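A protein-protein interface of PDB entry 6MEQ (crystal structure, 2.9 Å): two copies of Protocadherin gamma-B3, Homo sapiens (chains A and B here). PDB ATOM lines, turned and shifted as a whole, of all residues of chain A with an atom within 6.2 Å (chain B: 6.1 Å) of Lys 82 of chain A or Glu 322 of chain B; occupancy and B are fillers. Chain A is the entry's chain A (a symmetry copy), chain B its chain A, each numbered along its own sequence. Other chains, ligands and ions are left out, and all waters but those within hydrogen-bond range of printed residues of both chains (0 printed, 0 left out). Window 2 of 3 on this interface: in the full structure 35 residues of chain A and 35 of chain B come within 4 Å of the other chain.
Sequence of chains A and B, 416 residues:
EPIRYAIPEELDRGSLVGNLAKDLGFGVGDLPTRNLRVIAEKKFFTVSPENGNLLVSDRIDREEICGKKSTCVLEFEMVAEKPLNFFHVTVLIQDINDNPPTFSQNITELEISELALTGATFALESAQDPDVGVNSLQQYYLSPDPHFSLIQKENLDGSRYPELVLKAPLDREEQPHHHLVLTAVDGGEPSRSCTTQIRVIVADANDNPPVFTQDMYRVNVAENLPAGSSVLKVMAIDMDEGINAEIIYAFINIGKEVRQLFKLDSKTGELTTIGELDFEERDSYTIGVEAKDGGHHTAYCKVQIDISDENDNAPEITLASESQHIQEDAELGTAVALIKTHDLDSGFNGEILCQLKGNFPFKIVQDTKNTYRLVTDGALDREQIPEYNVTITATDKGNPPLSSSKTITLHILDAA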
ATOM      1  N   THR A  33     -29.381  31.214   2.634  1.00  0.00           N
ATOM      2  CA  THR A  33     -28.665  30.622   1.508  1.00  0.00           C
ATOM      3  C   THR A  33     -27.193  30.408   1.840  1.00  0.00           C
ATOM      4  O   THR A  33     -26.633  29.339   1.570  1.00  0.00           O
ATOM      5  CB  THR A  33     -28.813  31.505   0.267  1.00  0.00           C
ATOM      6  OG1 THR A  33     -30.200  31.624  -0.073  1.00  0.00           O
ATOM      7  CG2 THR A  33     -28.058  30.903  -0.909  1.00  0.00           C
ATOM      8  N   ARG A  34     -26.548  31.417   2.431  1.00  0.00           N
ATOM      9  CA  ARG A  34     -25.130  31.292   2.752  1.00  0.00           C
ATOM     10  C   ARG A  34     -24.902  30.402   3.966  1.00  0.00           C
ATOM     11  O   ARG A  34     -23.836  29.788   4.086  1.00  0.00           O
ATOM     12  CB  ARG A  34     -24.520  32.675   2.979  1.00  0.00           C
ATOM     13  CG  ARG A  34     -24.704  33.626   1.808  1.00  0.00           C
ATOM     14  CD  ARG A  34     -24.088  33.069   0.532  1.00  0.00           C
ATOM     15  NE  ARG A  34     -22.629  33.052   0.583  1.00  0.00           N
ATOM     16  CZ  ARG A  34     -21.857  34.047   0.157  1.00  0.00           C
ATOM     17  NH1 ARG A  34     -22.406  35.139  -0.355  1.00  0.00           N
ATOM     18  NH2 ARG A  34     -20.537  33.948   0.241  1.00  0.00           N
ATOM     19  N   ARG A  37     -21.814  29.906   9.805  1.00  0.00           N
ATOM     20  CA  ARG A  37     -21.485  29.086  10.961  1.00  0.00           C
ATOM     21  C   ARG A  37     -20.047  29.369  11.367  1.00  0.00           C
ATOM     22  O   ARG A  37     -19.201  29.685  10.525  1.00  0.00           O
ATOM     23  CB  ARG A  37     -21.678  27.594  10.669  1.00  0.00           C
ATOM     24  CG  ARG A  37     -20.833  27.065   9.522  1.00  0.00           C
ATOM     25  CD  ARG A  37     -21.098  25.588   9.279  1.00  0.00           C
ATOM     26  NE  ARG A  37     -20.284  25.056   8.190  1.00  0.00           N
ATOM     27  CZ  ARG A  37     -20.644  25.072   6.910  1.00  0.00           C
ATOM     28  NH1 ARG A  37     -21.807  25.599   6.554  1.00  0.00           N
ATOM     29  NH2 ARG A  37     -19.839  24.564   5.987  1.00  0.00           N
ATOM     30  N   ALA A  80     -19.026  30.360   4.996  1.00  0.00           N
ATOM     31  CA  ALA A  80     -20.227  30.597   4.211  1.00  0.00           C
ATOM     32  C   ALA A  80     -20.196  29.696   2.986  1.00  0.00           C
ATOM     33  O   ALA A  80     -19.131  29.464   2.407  1.00  0.00           O
ATOM     34  CB  ALA A  80     -20.338  32.063   3.783  1.00  0.00           C
ATOM     35  N   GLU A  81     -21.359  29.185   2.595  1.00  0.00           N
ATOM     36  CA  GLU A  81     -21.465  28.289   1.455  1.00  0.00           C
ATOM     37  C   GLU A  81     -22.318  28.921   0.362  1.00  0.00           C
ATOM     38  O   GLU A  81     -23.082  29.861   0.602  1.00  0.00           O
ATOM     39  CB  GLU A  81     -22.042  26.927   1.866  1.00  0.00           C
ATOM     40  CG  GLU A  81     -23.255  27.000   2.775  1.00  0.00           C
ATOM     41  CD  GLU A  81     -23.633  25.647   3.342  1.00  0.00           C
ATOM     42  OE1 GLU A  81     -23.215  24.623   2.766  1.00  0.00           O
ATOM     43  OE2 GLU A  81     -24.343  25.605   4.369  1.00  0.00           O
ATOM     44  N   LYS A  82     -22.167  28.385  -0.852  1.00  0.00           N
ATOM     45  CA  LYS A  82     -22.814  28.871  -2.066  1.00  0.00           C
ATOM     46  C   LYS A  82     -22.502  30.343  -2.313  1.00  0.00           C
ATOM     47  O   LYS A  82     -23.399  31.189  -2.201  1.00  0.00           O
ATOM     48  CB  LYS A  82     -24.331  28.670  -1.992  1.00  0.00           C
ATOM     49  CG  LYS A  82     -24.773  27.244  -1.717  1.00  0.00           C
ATOM     50  CD  LYS A  82     -26.289  27.166  -1.626  1.00  0.00           C
ATOM     51  CE  LYS A  82     -26.756  25.775  -1.236  1.00  0.00           C
ATOM     52  NZ  LYS A  82     -28.241  25.699  -1.140  1.00  0.00           N
ATOM     53  N   PRO A  83     -21.252  30.699  -2.657  1.00  0.00           N
ATOM     54  CA  PRO A  83     -20.083  29.821  -2.772  1.00  0.00           C
ATOM     55  C   PRO A  83     -19.356  29.651  -1.441  1.00  0.00           C
ATOM     56  O   PRO A  83     -19.702  30.319  -0.466  1.00  0.00           O
ATOM     57  CB  PRO A  83     -19.205  30.557  -3.780  1.00  0.00           C
ATOM     58  CG  PRO A  83     -19.488  31.993  -3.507  1.00  0.00           C
ATOM     59  CD  PRO A  83     -20.944  32.071  -3.101  1.00  0.00           C
ATOM     60  N   LEU A  84     -18.359  28.771  -1.404  1.00  0.00           N
ATOM     61  CA  LEU A  84     -17.592  28.515  -0.192  1.00  0.00           C
ATOM     62  C   LEU A  84     -16.450  29.518  -0.085  1.00  0.00           C
ATOM     63  O   LEU A  84     -15.627  29.631  -1.000  1.00  0.00           O
ATOM     64  CB  LEU A  84     -17.055  27.085  -0.182  1.00  0.00           C
ATOM     65  CG  LEU A  84     -18.033  26.011   0.294  1.00  0.00           C
ATOM     66  CD1 LEU A  84     -17.434  24.632   0.108  1.00  0.00           C
ATOM     67  CD2 LEU A  84     -18.400  26.239   1.750  1.00  0.00           C
ATOM     68  N   ALA B 320     -14.285  21.985   5.969  1.00  0.00           N
ATOM     69  CA  ALA B 320     -15.662  22.452   5.917  1.00  0.00           C
ATOM     70  C   ALA B 320     -16.138  22.388   4.473  1.00  0.00           C
ATOM     71  O   ALA B 320     -15.376  22.690   3.551  1.00  0.00           O
ATOM     72  CB  ALA B 320     -15.795  23.880   6.461  1.00  0.00           C
ATOM     73  N   SER B 321     -17.395  21.992   4.284  1.00  0.00           N
ATOM     74  CA  SER B 321     -17.955  21.837   2.949  1.00  0.00           C
ATOM     75  C   SER B 321     -19.466  22.014   3.018  1.00  0.00           C
ATOM     76  O   SER B 321     -20.038  22.258   4.085  1.00  0.00           O
ATOM     77  CB  SER B 321     -17.583  20.475   2.353  1.00  0.00           C
ATOM     78  OG  SER B 321     -18.086  19.417   3.149  1.00  0.00           O
ATOM     79  N   GLU B 322     -20.112  21.887   1.859  1.00  0.00           N
ATOM     80  CA  GLU B 322     -21.569  21.991   1.757  1.00  0.00           C
ATOM     81  C   GLU B 322     -22.191  20.622   2.040  1.00  0.00           C
ATOM     82  O   GLU B 322     -22.687  19.921   1.155  1.00  0.00           O
ATOM     83  CB  GLU B 322     -21.968  22.524   0.387  1.00  0.00           C
ATOM     84  CG  GLU B 322     -23.462  22.764   0.204  1.00  0.00           C
ATOM     85  CD  GLU B 322     -23.814  23.202  -1.204  1.00  0.00           C
ATOM     86  OE1 GLU B 322     -22.904  23.643  -1.937  1.00  0.00           O
ATOM     87  OE2 GLU B 322     -25.001  23.100  -1.580  1.00  0.00           O
ATOM     88  N   SER B 323     -22.135  20.242   3.319  1.00  0.00           N
ATOM     89  CA  SER B 323     -22.662  18.960   3.792  1.00  0.00           C
ATOM     90  C   SER B 323     -22.049  17.785   3.036  1.00  0.00           C
ATOM     91  O   SER B 323     -22.672  16.730   2.890  1.00  0.00           O
ATOM     92  CB  SER B 323     -24.191  18.924   3.701  1.00  0.00           C
ATOM     93  OG  SER B 323     -24.773  19.921   4.522  1.00  0.00           O
ATOM     94  N   GLN B 324     -20.820  17.970   2.547  1.00  0.00           N
ATOM     95  CA  GLN B 324     -20.080  16.931   1.827  1.00  0.00           C
ATOM     96  C   GLN B 324     -20.843  16.456   0.592  1.00  0.00           C
ATOM     97  O   GLN B 324     -20.868  15.265   0.275  1.00  0.00           O
ATOM     98  CB  GLN B 324     -19.746  15.755   2.748  1.00  0.00           C
ATOM     99  CG  GLN B 324     -18.996  16.150   4.011  1.00  0.00           C
ATOM    100  CD  GLN B 324     -18.818  14.990   4.971  1.00  0.00           C
ATOM    101  OE1 GLN B 324     -19.259  13.874   4.701  1.00  0.00           O
ATOM    102  NE2 GLN B 324     -18.171  15.252   6.101  1.00  0.00           N
ATOM    103  N   HIS B 325     -21.470  17.394  -0.113  1.00  0.00           N
ATOM    104  CA  HIS B 325     -22.251  17.098  -1.306  1.00  0.00           C
ATOM    105  C   HIS B 325     -21.715  17.890  -2.489  1.00  0.00           C
ATOM    106  O   HIS B 325     -21.402  19.079  -2.363  1.00  0.00           O
ATOM    107  CB  HIS B 325     -23.736  17.422  -1.095  1.00  0.00           C
ATOM    108  CG  HIS B 325     -24.423  16.510  -0.127  1.00  0.00           C
ATOM    109  ND1 HIS B 325     -25.696  16.751   0.345  1.00  0.00           N
ATOM    110  CD2 HIS B 325     -24.020  15.355   0.453  1.00  0.00           C
ATOM    111  CE1 HIS B 325     -26.045  15.785   1.177  1.00  0.00           C
ATOM    112  NE2 HIS B 325     -25.046  14.926   1.260  1.00  0.00           N
ATOM    113  N   ILE B 326     -21.611  17.225  -3.639  1.00  0.00           N
ATOM    114  CA  ILE B 326     -21.150  17.840  -4.876  1.00  0.00           C
ATOM    115  C   ILE B 326     -22.165  17.542  -5.970  1.00  0.00           C
ATOM    116  O   ILE B 326     -22.699  16.430  -6.048  1.00  0.00           O
ATOM    117  CB  ILE B 326     -19.753  17.331  -5.291  1.00  0.00           C
ATOM    118  CG1 ILE B 326     -18.770  17.405  -4.123  1.00  0.00           C
ATOM    119  CG2 ILE B 326     -19.218  18.129  -6.470  1.00  0.00           C
ATOM    120  CD1 ILE B 326     -17.409  16.834  -4.452  1.00  0.00           C
ATOM    121  N   GLN B 327     -22.430  18.535  -6.815  1.00  0.00           N
ATOM    122  CA  GLN B 327     -23.269  18.341  -7.987  1.00  0.00           C
ATOM    123  C   GLN B 327     -22.403  17.949  -9.178  1.00  0.00           C
ATOM    124  O   GLN B 327     -21.342  18.534  -9.408  1.00  0.00           O
ATOM    125  CB  GLN B 327     -24.063  19.610  -8.304  1.00  0.00           C
ATOM    126  CG  GLN B 327     -25.016  20.034  -7.198  1.00  0.00           C
ATOM    127  CD  GLN B 327     -25.874  21.221  -7.589  1.00  0.00           C
ATOM    128  OE1 GLN B 327     -25.855  21.665  -8.737  1.00  0.00           O
ATOM    129  NE2 GLN B 327     -26.633  21.742  -6.632  1.00  0.00           N
ATOM    130  N   VAL B 336     -15.161  23.289  -3.345  1.00  0.00           N
ATOM    131  CA  VAL B 336     -15.839  22.127  -2.795  1.00  0.00           C
ATOM    132  C   VAL B 336     -15.589  21.985  -1.298  1.00  0.00           C
ATOM    133  O   VAL B 336     -16.509  21.666  -0.541  1.00  0.00           O
ATOM    134  CB  VAL B 336     -15.423  20.846  -3.549  1.00  0.00           C
ATOM    135  CG1 VAL B 336     -15.847  19.610  -2.779  1.00  0.00           C
ATOM    136  CG2 VAL B 336     -16.031  20.838  -4.940  1.00  0.00           C
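Printed residues of chain A that touch a printed residue of chain B: Arg 37, Glu 81, Lys 82 and Leu 84.
No position is printed for both chains.
Of the 4 pairs that touch across the chains among the printed residues, none has its exchanged pair printed and touching as well.
The guanidinium group (NH2) of Arg 37 of chain A lies within hydrogen-bond range of the backbone carbonyl oxygen (O) of Ser 321 of chain B.
Among the printed residues, merely in contact across the chains: Leu 84 of chain A with Val 336 of chain B (3.2 Å), Glu 81 of chain A with Glu 322 of chain B (3.2 Å) and Lys 82 of chain A with Glu 322 of chain B (3.2 Å).
Printed residues of chain B within 4 Å of Glu 81 of chain A: Glu 322 (3.2 Å).
Printed residues of chain A within 4 Å of Ser 321 of chain B: Arg 37.
Of chain A, only Glu 81 and Lys 82 come within 4 Å of Glu 322 of chain B.
The nearest residue of chain A that does not touch Glu 322 of chain B is Leu 84 of chain A (4.2 Å).
The guanidinium group of Arg 37 of chain A is in salt-bridge range of the side-chain carboxylate of Glu 81 of chain A (3.3 Å).
The backbone carbonyl oxygen (O) of Arg 34 of chain A lies within hydrogen-bond range of the backbone NH (N) of Glu 81 of chain A, 3.0 Å away.
N of Gln 324 of chain B is in hydrogen-bond range of OG of Ser 321 of chain B.
The guanidinium group (NE) of Arg 34 of chain A lies close to the backbone carbonyl oxygen (O) of Lys 82 of chain A, 3.4 Å away.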
